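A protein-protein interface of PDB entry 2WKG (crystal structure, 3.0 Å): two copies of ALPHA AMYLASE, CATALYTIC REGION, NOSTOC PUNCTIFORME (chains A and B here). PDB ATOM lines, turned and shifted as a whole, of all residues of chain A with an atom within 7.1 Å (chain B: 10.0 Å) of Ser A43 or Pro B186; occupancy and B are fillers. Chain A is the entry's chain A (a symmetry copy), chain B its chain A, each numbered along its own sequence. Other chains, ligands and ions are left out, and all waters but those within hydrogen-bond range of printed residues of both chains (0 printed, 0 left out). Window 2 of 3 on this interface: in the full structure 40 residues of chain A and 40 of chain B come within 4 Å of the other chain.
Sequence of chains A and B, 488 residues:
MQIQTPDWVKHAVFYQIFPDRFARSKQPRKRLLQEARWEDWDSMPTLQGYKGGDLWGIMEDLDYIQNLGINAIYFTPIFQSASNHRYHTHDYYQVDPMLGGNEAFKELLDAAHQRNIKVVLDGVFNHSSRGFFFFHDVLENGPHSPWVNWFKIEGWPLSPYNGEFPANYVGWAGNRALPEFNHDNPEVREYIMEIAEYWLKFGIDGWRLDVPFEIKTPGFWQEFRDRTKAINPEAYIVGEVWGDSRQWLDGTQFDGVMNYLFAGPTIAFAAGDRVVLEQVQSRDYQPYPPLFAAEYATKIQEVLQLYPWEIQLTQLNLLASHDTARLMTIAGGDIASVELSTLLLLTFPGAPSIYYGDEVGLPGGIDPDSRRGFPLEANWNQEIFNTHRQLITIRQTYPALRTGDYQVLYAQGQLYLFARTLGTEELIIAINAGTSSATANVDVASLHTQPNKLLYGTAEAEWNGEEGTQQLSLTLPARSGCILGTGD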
ATOM      1  N   LEU A  33     -21.449  22.434  27.193  1.00  0.00           N
ATOM      2  CA  LEU A  33     -20.571  22.791  28.303  1.00  0.00           C
ATOM      3  C   LEU A  33     -20.828  24.219  28.771  1.00  0.00           C
ATOM      4  O   LEU A  33     -20.176  25.159  28.312  1.00  0.00           O
ATOM      5  CB  LEU A  33     -19.106  22.623  27.901  1.00  0.00           C
ATOM      6  CG  LEU A  33     -18.743  21.322  27.184  1.00  0.00           C
ATOM      7  CD1 LEU A  33     -19.614  20.176  27.678  1.00  0.00           C
ATOM      8  CD2 LEU A  33     -18.869  21.485  25.677  1.00  0.00           C
ATOM      9  N   ARG A  37     -14.956  28.444  28.818  1.00  0.00           N
ATOM     10  CA  ARG A  37     -14.347  29.706  28.415  1.00  0.00           C
ATOM     11  C   ARG A  37     -14.831  30.136  27.034  1.00  0.00           C
ATOM     12  O   ARG A  37     -14.655  29.414  26.051  1.00  0.00           O
ATOM     13  CB  ARG A  37     -12.821  29.593  28.426  1.00  0.00           C
ATOM     14  CG  ARG A  37     -12.219  29.449  29.813  1.00  0.00           C
ATOM     15  CD  ARG A  37     -12.314  30.749  30.595  1.00  0.00           C
ATOM     16  NE  ARG A  37     -11.606  30.674  31.869  1.00  0.00           N
ATOM     17  CZ  ARG A  37     -11.458  31.699  32.704  1.00  0.00           C
ATOM     18  NH1 ARG A  37     -11.971  32.883  32.399  1.00  0.00           N
ATOM     19  NH2 ARG A  37     -10.799  31.539  33.842  1.00  0.00           N
ATOM     20  N   GLU A  39     -13.408  31.971  25.386  1.00  0.00           N
ATOM     21  CA  GLU A  39     -12.162  32.102  24.641  1.00  0.00           C
ATOM     22  C   GLU A  39     -11.740  30.767  24.035  1.00  0.00           C
ATOM     23  O   GLU A  39     -11.037  30.729  23.025  1.00  0.00           O
ATOM     24  CB  GLU A  39     -11.052  32.644  25.543  1.00  0.00           C
ATOM     25  CG  GLU A  39     -11.533  33.630  26.596  1.00  0.00           C
ATOM     26  CD  GLU A  39     -10.508  33.865  27.687  1.00  0.00           C
ATOM     27  OE1 GLU A  39      -9.928  32.875  28.181  1.00  0.00           O
ATOM     28  OE2 GLU A  39     -10.282  35.038  28.049  1.00  0.00           O
ATOM     29  N   ASP A  40     -12.172  29.677  24.658  1.00  0.00           N
ATOM     30  CA  ASP A  40     -11.947  28.343  24.114  1.00  0.00           C
ATOM     31  C   ASP A  40     -13.132  27.886  23.271  1.00  0.00           C
ATOM     32  O   ASP A  40     -13.115  26.796  22.698  1.00  0.00           O
ATOM     33  CB  ASP A  40     -11.685  27.341  25.241  1.00  0.00           C
ATOM     34  CG  ASP A  40     -10.593  27.802  26.187  1.00  0.00           C
ATOM     35  OD1 ASP A  40     -10.687  28.938  26.697  1.00  0.00           O
ATOM     36  OD2 ASP A  40      -9.641  27.028  26.419  1.00  0.00           O
ATOM     37  N   TRP A  41     -14.160  28.724  23.200  1.00  0.00           N
ATOM     38  CA  TRP A  41     -15.432  28.328  22.604  1.00  0.00           C
ATOM     39  C   TRP A  41     -15.236  27.794  21.190  1.00  0.00           C
ATOM     40  O   TRP A  41     -15.673  26.690  20.867  1.00  0.00           O
ATOM     41  CB  TRP A  41     -16.407  29.507  22.591  1.00  0.00           C
ATOM     42  CG  TRP A  41     -17.642  29.257  21.782  1.00  0.00           C
ATOM     43  CD1 TRP A  41     -17.779  29.396  20.431  1.00  0.00           C
ATOM     44  CD2 TRP A  41     -18.916  28.821  22.271  1.00  0.00           C
ATOM     45  NE1 TRP A  41     -19.059  29.075  20.049  1.00  0.00           N
ATOM     46  CE2 TRP A  41     -19.778  28.718  21.161  1.00  0.00           C
ATOM     47  CE3 TRP A  41     -19.413  28.507  23.540  1.00  0.00           C
ATOM     48  CZ2 TRP A  41     -21.105  28.315  21.281  1.00  0.00           C
ATOM     49  CZ3 TRP A  41     -20.731  28.108  23.658  1.00  0.00           C
ATOM     50  CH2 TRP A  41     -21.562  28.016  22.533  1.00  0.00           C
ATOM     51  N   ASP A  42     -14.577  28.586  20.349  1.00  0.00           N
ATOM     52  CA  ASP A  42     -14.367  28.217  18.955  1.00  0.00           C
ATOM     53  C   ASP A  42     -13.578  26.917  18.842  1.00  0.00           C
ATOM     54  O   ASP A  42     -13.638  26.231  17.822  1.00  0.00           O
ATOM     55  CB  ASP A  42     -13.643  29.339  18.207  1.00  0.00           C
ATOM     56  CG  ASP A  42     -13.716  29.177  16.702  1.00  0.00           C
ATOM     57  OD1 ASP A  42     -13.312  28.108  16.197  1.00  0.00           O
ATOM     58  OD2 ASP A  42     -14.178  30.119  16.023  1.00  0.00           O
ATOM     59  N   SER A  43     -12.839  26.586  19.895  1.00  0.00           N
ATOM     60  CA  SER A  43     -12.097  25.331  19.947  1.00  0.00           C
ATOM     61  C   SER A  43     -13.038  24.133  19.893  1.00  0.00           C
ATOM     62  O   SER A  43     -12.661  23.054  19.433  1.00  0.00           O
ATOM     63  CB  SER A  43     -11.239  25.269  21.212  1.00  0.00           C
ATOM     64  OG  SER A  43     -10.705  26.541  21.530  1.00  0.00           O
ATOM     65  N   MET A  44     -14.266  24.327  20.363  1.00  0.00           N
ATOM     66  CA  MET A  44     -15.261  23.262  20.372  1.00  0.00           C
ATOM     67  C   MET A  44     -16.291  23.463  19.266  1.00  0.00           C
ATOM     68  O   MET A  44     -17.245  24.225  19.422  1.00  0.00           O
ATOM     69  CB  MET A  44     -15.958  23.191  21.732  1.00  0.00           C
ATOM     70  CG  MET A  44     -15.004  23.126  22.914  1.00  0.00           C
ATOM     71  SD  MET A  44     -15.789  23.598  24.468  1.00  0.00           S
ATOM     72  CE  MET A  44     -14.876  25.085  24.870  1.00  0.00           C
ATOM     73  N   PRO A  45     -16.093  22.771  18.147  1.00  0.00           N
ATOM     74  CA  PRO A  45     -16.892  23.012  16.942  1.00  0.00           C
ATOM     75  C   PRO A  45     -18.378  22.764  17.188  1.00  0.00           C
ATOM     76  O   PRO A  45     -19.209  23.596  16.825  1.00  0.00           O
ATOM     77  CB  PRO A  45     -16.345  21.979  15.954  1.00  0.00           C
ATOM     78  CG  PRO A  45     -14.940  21.761  16.389  1.00  0.00           C
ATOM     79  CD  PRO A  45     -14.949  21.881  17.886  1.00  0.00           C
ATOM     80  N   THR A  46     -18.699  21.631  17.802  1.00  0.00           N
ATOM     81  CA  THR A  46     -20.089  21.231  17.992  1.00  0.00           C
ATOM     82  C   THR A  46     -20.916  22.372  18.575  1.00  0.00           C
ATOM     83  O   THR A  46     -22.012  22.664  18.098  1.00  0.00           O
ATOM     84  CB  THR A  46     -20.201  20.003  18.915  1.00  0.00           C
ATOM     85  OG1 THR A  46     -19.724  18.840  18.228  1.00  0.00           O
ATOM     86  CG2 THR A  46     -21.647  19.782  19.333  1.00  0.00           C
ATOM     87  N   GLN A  48     -19.766  25.540  18.811  1.00  0.00           N
ATOM     88  CA  GLN A  48     -19.458  26.747  18.053  1.00  0.00           C
ATOM     89  C   GLN A  48     -20.563  27.063  17.049  1.00  0.00           C
ATOM     90  O   GLN A  48     -21.152  28.143  17.080  1.00  0.00           O
ATOM     91  CB  GLN A  48     -18.118  26.599  17.330  1.00  0.00           C
ATOM     92  CG  GLN A  48     -17.853  27.672  16.287  1.00  0.00           C
ATOM     93  CD  GLN A  48     -17.677  27.100  14.894  1.00  0.00           C
ATOM     94  OE1 GLN A  48     -18.649  26.741  14.230  1.00  0.00           O
ATOM     95  NE2 GLN A  48     -16.431  27.011  14.444  1.00  0.00           N
ATOM     96  N   ASN B 149     -16.060  12.406  16.998  1.00  0.00           N
ATOM     97  CA  ASN B 149     -14.736  12.920  17.306  1.00  0.00           C
ATOM     98  C   ASN B 149     -14.571  13.091  18.818  1.00  0.00           C
ATOM     99  O   ASN B 149     -13.753  13.879  19.282  1.00  0.00           O
ATOM    100  CB  ASN B 149     -14.531  14.254  16.580  1.00  0.00           C
ATOM    101  CG  ASN B 149     -13.171  14.872  16.851  1.00  0.00           C
ATOM    102  OD1 ASN B 149     -12.137  14.213  16.725  1.00  0.00           O
ATOM    103  ND2 ASN B 149     -13.165  16.153  17.216  1.00  0.00           N
ATOM    104  N   TRP B 150     -15.365  12.352  19.587  1.00  0.00           N
ATOM    105  CA  TRP B 150     -15.287  12.407  21.046  1.00  0.00           C
ATOM    106  C   TRP B 150     -14.611  11.141  21.529  1.00  0.00           C
ATOM    107  O   TRP B 150     -14.175  11.063  22.671  1.00  0.00           O
ATOM    108  CB  TRP B 150     -16.687  12.510  21.676  1.00  0.00           C
ATOM    109  CG  TRP B 150     -17.093  13.914  22.008  1.00  0.00           C
ATOM    110  CD1 TRP B 150     -16.983  15.007  21.201  1.00  0.00           C
ATOM    111  CD2 TRP B 150     -17.650  14.384  23.242  1.00  0.00           C
ATOM    112  NE1 TRP B 150     -17.431  16.133  21.852  1.00  0.00           N
ATOM    113  CE2 TRP B 150     -17.847  15.781  23.109  1.00  0.00           C
ATOM    114  CE3 TRP B 150     -18.002  13.765  24.450  1.00  0.00           C
ATOM    115  CZ2 TRP B 150     -18.380  16.571  24.141  1.00  0.00           C
ATOM    116  CZ3 TRP B 150     -18.533  14.554  25.476  1.00  0.00           C
ATOM    117  CH2 TRP B 150     -18.715  15.940  25.311  1.00  0.00           C
ATOM    118  N   PHE B 181     -12.101   7.881  25.811  1.00  0.00           N
ATOM    119  CA  PHE B 181     -12.408   9.234  25.360  1.00  0.00           C
ATOM    120  C   PHE B 181     -11.252   9.733  24.489  1.00  0.00           C
ATOM    121  O   PHE B 181     -10.158   9.170  24.492  1.00  0.00           O
ATOM    122  CB  PHE B 181     -12.566  10.208  26.545  1.00  0.00           C
ATOM    123  CG  PHE B 181     -13.846  10.046  27.326  1.00  0.00           C
ATOM    124  CD1 PHE B 181     -13.952   9.103  28.340  1.00  0.00           C
ATOM    125  CD2 PHE B 181     -14.941  10.857  27.065  1.00  0.00           C
ATOM    126  CE1 PHE B 181     -15.131   8.975  29.084  1.00  0.00           C
ATOM    127  CE2 PHE B 181     -16.118  10.731  27.805  1.00  0.00           C
ATOM    128  CZ  PHE B 181     -16.209   9.790  28.814  1.00  0.00           C
ATOM    129  N   ASN B 182     -11.503  10.796  23.742  1.00  0.00           N
ATOM    130  CA  ASN B 182     -10.481  11.392  22.901  1.00  0.00           C
ATOM    131  C   ASN B 182     -10.084  12.664  23.626  1.00  0.00           C
ATOM    132  O   ASN B 182     -10.543  13.758  23.305  1.00  0.00           O
ATOM    133  CB  ASN B 182     -11.052  11.707  21.521  1.00  0.00           C
ATOM    134  CG  ASN B 182     -10.130  12.572  20.706  1.00  0.00           C
ATOM    135  OD1 ASN B 182      -8.916  12.562  20.911  1.00  0.00           O
ATOM    136  ND2 ASN B 182     -10.695  13.320  19.767  1.00  0.00           N
ATOM    137  N   HIS B 183      -9.227  12.500  24.623  1.00  0.00           N
ATOM    138  CA  HIS B 183      -8.789  13.612  25.445  1.00  0.00           C
ATOM    139  C   HIS B 183      -8.181  14.795  24.714  1.00  0.00           C
ATOM    140  O   HIS B 183      -8.154  15.905  25.248  1.00  0.00           O
ATOM    141  CB  HIS B 183      -7.838  13.094  26.515  1.00  0.00           C
ATOM    142  CG  HIS B 183      -8.472  12.100  27.436  1.00  0.00           C
ATOM    143  ND1 HIS B 183      -8.789  10.819  27.041  1.00  0.00           N
ATOM    144  CD2 HIS B 183      -8.901  12.217  28.714  1.00  0.00           C
ATOM    145  CE1 HIS B 183      -9.387  10.190  28.037  1.00  0.00           C
ATOM    146  NE2 HIS B 183      -9.467  11.016  29.064  1.00  0.00           N
ATOM    147  N   ASP B 184      -7.695  14.572  23.498  1.00  0.00           N
ATOM    148  CA  ASP B 184      -7.112  15.661  22.720  1.00  0.00           C
ATOM    149  C   ASP B 184      -8.202  16.666  22.373  1.00  0.00           C
ATOM    150  O   ASP B 184      -7.942  17.864  22.262  1.00  0.00           O
ATOM    151  CB  ASP B 184      -6.473  15.125  21.435  1.00  0.00           C
ATOM    152  CG  ASP B 184      -5.105  14.501  21.676  1.00  0.00           C
ATOM    153  OD1 ASP B 184      -4.579  13.843  20.752  1.00  0.00           O
ATOM    154  OD2 ASP B 184      -4.548  14.679  22.781  1.00  0.00           O
ATOM    155  N   ASN B 185      -9.426  16.162  22.223  1.00  0.00           N
ATOM    156  CA  ASN B 185     -10.591  16.980  21.885  1.00  0.00           C
ATOM    157  C   ASN B 185     -10.960  17.967  23.003  1.00  0.00           C
ATOM    158  O   ASN B 185     -11.346  17.569  24.105  1.00  0.00           O
ATOM    159  CB  ASN B 185     -11.789  16.076  21.588  1.00  0.00           C
ATOM    160  CG  ASN B 185     -12.941  16.826  20.960  1.00  0.00           C
ATOM    161  OD1 ASN B 185     -13.267  17.940  21.364  1.00  0.00           O
ATOM    162  ND2 ASN B 185     -13.574  16.213  19.973  1.00  0.00           N
ATOM    163  N   PRO B 186     -10.852  19.273  22.721  1.00  0.00           N
ATOM    164  CA  PRO B 186     -11.160  20.348  23.669  1.00  0.00           C
ATOM    165  C   PRO B 186     -12.503  20.169  24.361  1.00  0.00           C
ATOM    166  O   PRO B 186     -12.618  20.346  25.575  1.00  0.00           O
ATOM    167  CB  PRO B 186     -11.137  21.593  22.789  1.00  0.00           C
ATOM    168  CG  PRO B 186     -10.095  21.257  21.788  1.00  0.00           C
ATOM    169  CD  PRO B 186     -10.441  19.833  21.422  1.00  0.00           C
ATOM    170  N   GLU B 187     -13.512  19.824  23.569  1.00  0.00           N
ATOM    171  CA  GLU B 187     -14.868  19.623  24.063  1.00  0.00           C
ATOM    172  C   GLU B 187     -14.891  18.589  25.170  1.00  0.00           C
ATOM    173  O   GLU B 187     -15.627  18.723  26.145  1.00  0.00           O
ATOM    174  CB  GLU B 187     -15.770  19.165  22.923  1.00  0.00           C
ATOM    175  CG  GLU B 187     -15.661  20.031  21.695  1.00  0.00           C
ATOM    176  CD  GLU B 187     -16.791  19.793  20.727  1.00  0.00           C
ATOM    177  OE1 GLU B 187     -16.988  18.629  20.323  1.00  0.00           O
ATOM    178  OE2 GLU B 187     -17.480  20.772  20.373  1.00  0.00           O
ATOM    179  N   VAL B 188     -14.075  17.558  25.003  1.00  0.00           N
ATOM    180  CA  VAL B 188     -13.967  16.478  25.969  1.00  0.00           C
ATOM    181  C   VAL B 188     -13.259  16.935  27.249  1.00  0.00           C
ATOM    182  O   VAL B 188     -13.737  16.674  28.356  1.00  0.00           O
ATOM    183  CB  VAL B 188     -13.212  15.299  25.343  1.00  0.00           C
ATOM    184  CG1 VAL B 188     -13.074  14.164  26.338  1.00  0.00           C
ATOM    185  CG2 VAL B 188     -13.945  14.846  24.091  1.00  0.00           C
ATOM    186  N   ARG B 189     -12.126  17.617  27.099  1.00  0.00           N
ATOM    187  CA  ARG B 189     -11.386  18.104  28.261  1.00  0.00           C
ATOM    188  C   ARG B 189     -12.332  18.958  29.089  1.00  0.00           C
ATOM    189  O   ARG B 189     -12.285  18.952  30.320  1.00  0.00           O
ATOM    190  CB  ARG B 189     -10.173  18.944  27.831  1.00  0.00           C
ATOM    191  CG  ARG B 189      -9.075  18.163  27.106  1.00  0.00           C
ATOM    192  CD  ARG B 189      -8.271  19.057  26.143  1.00  0.00           C
ATOM    193  NE  ARG B 189      -6.967  19.461  26.668  1.00  0.00           N
ATOM    194  CZ  ARG B 189      -6.782  20.133  27.801  1.00  0.00           C
ATOM    195  NH1 ARG B 189      -7.820  20.487  28.545  1.00  0.00           N
ATOM    196  NH2 ARG B 189      -5.552  20.451  28.186  1.00  0.00           N
ATOM    197  N   GLU B 190     -13.204  19.682  28.397  1.00  0.00           N
ATOM    198  CA  GLU B 190     -14.171  20.549  29.054  1.00  0.00           C
ATOM    199  C   GLU B 190     -15.202  19.774  29.862  1.00  0.00           C
ATOM    200  O   GLU B 190     -15.382  20.018  31.054  1.00  0.00           O
ATOM    201  CB  GLU B 190     -14.893  21.407  28.021  1.00  0.00           C
ATOM    202  CG  GLU B 190     -14.613  22.867  28.187  1.00  0.00           C
ATOM    203  CD  GLU B 190     -14.779  23.302  29.621  1.00  0.00           C
ATOM    204  OE1 GLU B 190     -15.918  23.264  30.132  1.00  0.00           O
ATOM    205  OE2 GLU B 190     -13.761  23.671  30.239  1.00  0.00           O
ATOM    206  N   TYR B 191     -15.879  18.842  29.197  1.00  0.00           N
ATOM    207  CA  TYR B 191     -16.902  18.027  29.834  1.00  0.00           C
ATOM    208  C   TYR B 191     -16.349  17.350  31.074  1.00  0.00           C
ATOM    209  O   TYR B 191     -17.043  17.223  32.085  1.00  0.00           O
ATOM    210  CB  TYR B 191     -17.423  16.984  28.842  1.00  0.00           C
ATOM    211  CG  TYR B 191     -18.509  16.073  29.384  1.00  0.00           C
ATOM    212  CD1 TYR B 191     -18.205  14.791  29.840  1.00  0.00           C
ATOM    213  CD2 TYR B 191     -19.844  16.481  29.414  1.00  0.00           C
ATOM    214  CE1 TYR B 191     -19.197  13.937  30.305  1.00  0.00           C
ATOM    215  CE2 TYR B 191     -20.846  15.631  29.882  1.00  0.00           C
ATOM    216  CZ  TYR B 191     -20.514  14.360  30.323  1.00  0.00           C
ATOM    217  OH  TYR B 191     -21.494  13.504  30.775  1.00  0.00           O
ATOM    218  N   ILE B 192     -15.094  16.924  30.996  1.00  0.00           N
ATOM    219  CA  ILE B 192     -14.464  16.262  32.125  1.00  0.00           C
ATOM    220  C   ILE B 192     -14.171  17.253  33.247  1.00  0.00           C
ATOM    221  O   ILE B 192     -14.459  16.985  34.413  1.00  0.00           O
ATOM    222  CB  ILE B 192     -13.154  15.553  31.700  1.00  0.00           C
ATOM    223  CG1 ILE B 192     -13.486  14.374  30.775  1.00  0.00           C
ATOM    224  CG2 ILE B 192     -12.403  15.060  32.921  1.00  0.00           C
ATOM    225  CD1 ILE B 192     -12.306  13.496  30.414  1.00  0.00           C
ATOM    226  N   MET B 193     -13.611  18.405  32.899  1.00  0.00           N
ATOM    227  CA  MET B 193     -13.294  19.401  33.907  1.00  0.00           C
ATOM    228  C   MET B 193     -14.532  19.777  34.695  1.00  0.00           C
ATOM    229  O   MET B 193     -14.457  20.026  35.897  1.00  0.00           O
ATOM    230  CB  MET B 193     -12.703  20.644  33.259  1.00  0.00           C
ATOM    231  CG  MET B 193     -11.365  20.417  32.582  1.00  0.00           C
ATOM    232  SD  MET B 193     -10.067  19.933  33.730  1.00  0.00           S
ATOM    233  CE  MET B 193      -9.327  18.570  32.843  1.00  0.00           C
ATOM    234  N   GLU B 194     -15.675  19.812  34.016  1.00  0.00           N
ATOM    235  CA  GLU B 194     -16.937  20.170  34.656  1.00  0.00           C
ATOM    236  C   GLU B 194     -17.425  19.109  35.640  1.00  0.00           C
ATOM    237  O   GLU B 194     -17.952  19.439  36.699  1.00  0.00           O
ATOM    238  CB  GLU B 194     -17.997  20.444  33.590  1.00  0.00           C
ATOM    239  CG  GLU B 194     -17.815  21.795  32.905  1.00  0.00           C
ATOM    240  CD  GLU B 194     -18.705  21.975  31.692  1.00  0.00           C
ATOM    241  OE1 GLU B 194     -19.924  21.746  31.802  1.00  0.00           O
ATOM    242  OE2 GLU B 194     -18.185  22.356  30.627  1.00  0.00           O
ATOM    243  N   THR B 217      -2.873  13.828  26.926  1.00  0.00           N
ATOM    244  CA  THR B 217      -3.001  15.145  26.320  1.00  0.00           C
ATOM    245  C   THR B 217      -2.265  16.180  27.157  1.00  0.00           C
ATOM    246  O   THR B 217      -2.596  16.414  28.317  1.00  0.00           O
ATOM    247  CB  THR B 217      -4.463  15.565  26.191  1.00  0.00           C
ATOM    248  OG1 THR B 217      -5.140  14.642  25.330  1.00  0.00           O
ATOM    249  CG2 THR B 217      -4.559  16.973  25.616  1.00  0.00           C
ATOM    250  N   PRO B 218      -1.243  16.812  26.572  1.00  0.00           N
ATOM    251  CA  PRO B 218      -0.449  17.830  27.264  1.00  0.00           C
ATOM    252  C   PRO B 218      -1.232  19.013  27.822  1.00  0.00           C
ATOM    253  O   PRO B 218      -2.035  19.628  27.123  1.00  0.00           O
ATOM    254  CB  PRO B 218       0.581  18.247  26.207  1.00  0.00           C
ATOM    255  CG  PRO B 218      -0.086  17.902  24.899  1.00  0.00           C
ATOM    256  CD  PRO B 218      -0.728  16.578  25.212  1.00  0.00           C
ATOM    257  N   PHE B 220      -3.337  18.813  30.263  1.00  0.00           N
ATOM    258  CA  PHE B 220      -4.544  18.277  30.876  1.00  0.00           C
ATOM    259  C   PHE B 220      -4.597  18.412  32.402  1.00  0.00           C
ATOM    260  O   PHE B 220      -5.309  19.265  32.938  1.00  0.00           O
ATOM    261  CB  PHE B 220      -4.695  16.806  30.471  1.00  0.00           C
ATOM    262  CG  PHE B 220      -6.078  16.264  30.649  1.00  0.00           C
ATOM    263  CD1 PHE B 220      -6.587  16.013  31.916  1.00  0.00           C
ATOM    264  CD2 PHE B 220      -6.891  16.030  29.542  1.00  0.00           C
ATOM    265  CE1 PHE B 220      -7.884  15.540  32.079  1.00  0.00           C
ATOM    266  CE2 PHE B 220      -8.198  15.555  29.698  1.00  0.00           C
ATOM    267  CZ  PHE B 220      -8.692  15.312  30.969  1.00  0.00           C
ATOM    268  N   GLU B 223      -4.507  21.728  34.174  1.00  0.00           N
ATOM    269  CA  GLU B 223      -5.794  22.403  34.099  1.00  0.00           C
ATOM    270  C   GLU B 223      -6.711  21.792  35.140  1.00  0.00           C
ATOM    271  O   GLU B 223      -7.396  22.504  35.874  1.00  0.00           O
ATOM    272  CB  GLU B 223      -6.392  22.234  32.705  1.00  0.00           C
ATOM    273  CG  GLU B 223      -7.695  22.981  32.501  1.00  0.00           C
ATOM    274  CD  GLU B 223      -8.139  22.983  31.052  1.00  0.00           C
ATOM    275  OE1 GLU B 223      -9.203  23.561  30.756  1.00  0.00           O
ATOM    276  OE2 GLU B 223      -7.423  22.405  30.208  1.00  0.00           O
ATOM    277  N   ARG B 227      -8.710  24.212  37.806  1.00  0.00           N
ATOM    278  CA  ARG B 227     -10.163  24.250  37.876  1.00  0.00           C
ATOM    279  C   ARG B 227     -10.670  23.634  39.178  1.00  0.00           C
ATOM    280  O   ARG B 227     -11.690  24.069  39.721  1.00  0.00           O
ATOM    281  CB  ARG B 227     -10.755  23.515  36.673  1.00  0.00           C
ATOM    282  CG  ARG B 227     -10.603  24.277  35.360  1.00  0.00           C
ATOM    283  CD  ARG B 227     -10.828  23.372  34.152  1.00  0.00           C
ATOM    284  NE  ARG B 227     -11.784  23.924  33.190  1.00  0.00           N
ATOM    285  CZ  ARG B 227     -13.093  24.004  33.404  1.00  0.00           C
ATOM    286  NH1 ARG B 227     -13.609  23.570  34.539  1.00  0.00           N
ATOM    287  NH2 ARG B 227     -13.892  24.521  32.484  1.00  0.00           N
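No position is printed for both chains.
Among the printed residues, merely in contact across the chains: Leu A33 with Glu B190, Leu A33 with Glu B194, Ser A43 with Pro B186, Met A44 with Glu B187 and Met A44 with Glu B190.
The side-chain carboxylate (OE1) of Glu B187 lies within hydrogen-bond range of the indole nitrogen (NE1) of Trp B150 (3.0 Å).
OD1 of Asn B185 sits at hydrogen-bond distance from N of Glu B187 (2.9 Å).
OE1 of Glu B190 sits close to OE2 of Glu B194 (2.5 Å).
OE2 of Glu B190 is in salt-bridge range of NH2 of Arg B227 (2.4 Å).
The side-chain hydroxyl of Ser A43 is in hydrogen-bond range of the backbone carbonyl oxygen of Asp A40 (2.7 Å).
The side-chain carboxylate of Glu B187 is in hydrogen-bond range of the backbone NH of Thr A46 (3.0 Å).
The backbone nitrogen (N) of Pro A45 lies close to the side-chain carboxylate (OE2) of Glu B187, at 3.3 Å.
Ser A43 touches one residue of chain B.
Of chain A, only Ser A43 comes within 4 Å of Pro B186.
No residue of chain B comes within 4 Å of Asp A42.
Of chain B, only Glu B187 (3.1 Å) and Glu B190 (3.97 Å) come within 4 Å of Met A44.
Printed residues of chain A within 4 Å of Glu B187: Met A44, Pro A45 and Thr A46.
Printed residues of chain B within 4 Å of Pro A45: Glu B187.
Of the printed residues of chain B, Thr A46 touches Glu B187 (3.0 Å).
Printed residues of chain A within 4 Å of Glu B190: Leu A33 (3.9 Å) and Met A44 (3.97 Å).
Printed residues of chain B within 4 Å of Leu A33: Glu B190 and Glu B194.
The nearest residue of chain A that does not touch Pro B186 is Met A44 (4.1 Å).
The nearest printed residue of chain A that does not touch Glu B194 is Met A44 (6.7 Å).
Of the 11 printed residues of chain A, 5 touch a printed residue of chain B.
Printed residues of chain A that touch a printed residue of chain B: Leu A33, Ser A43, Met A44, Pro A45 and Thr A46.
Along chain B the printed residues that touch a printed residue of chain A span positions 186 to 194.
Among the printed residues, 7 pairs touch across the chains.
Among the printed residues, no Asp or Glu carboxylate lies within 4 Å of a Lys or Arg side-chain nitrogen of the other chain.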
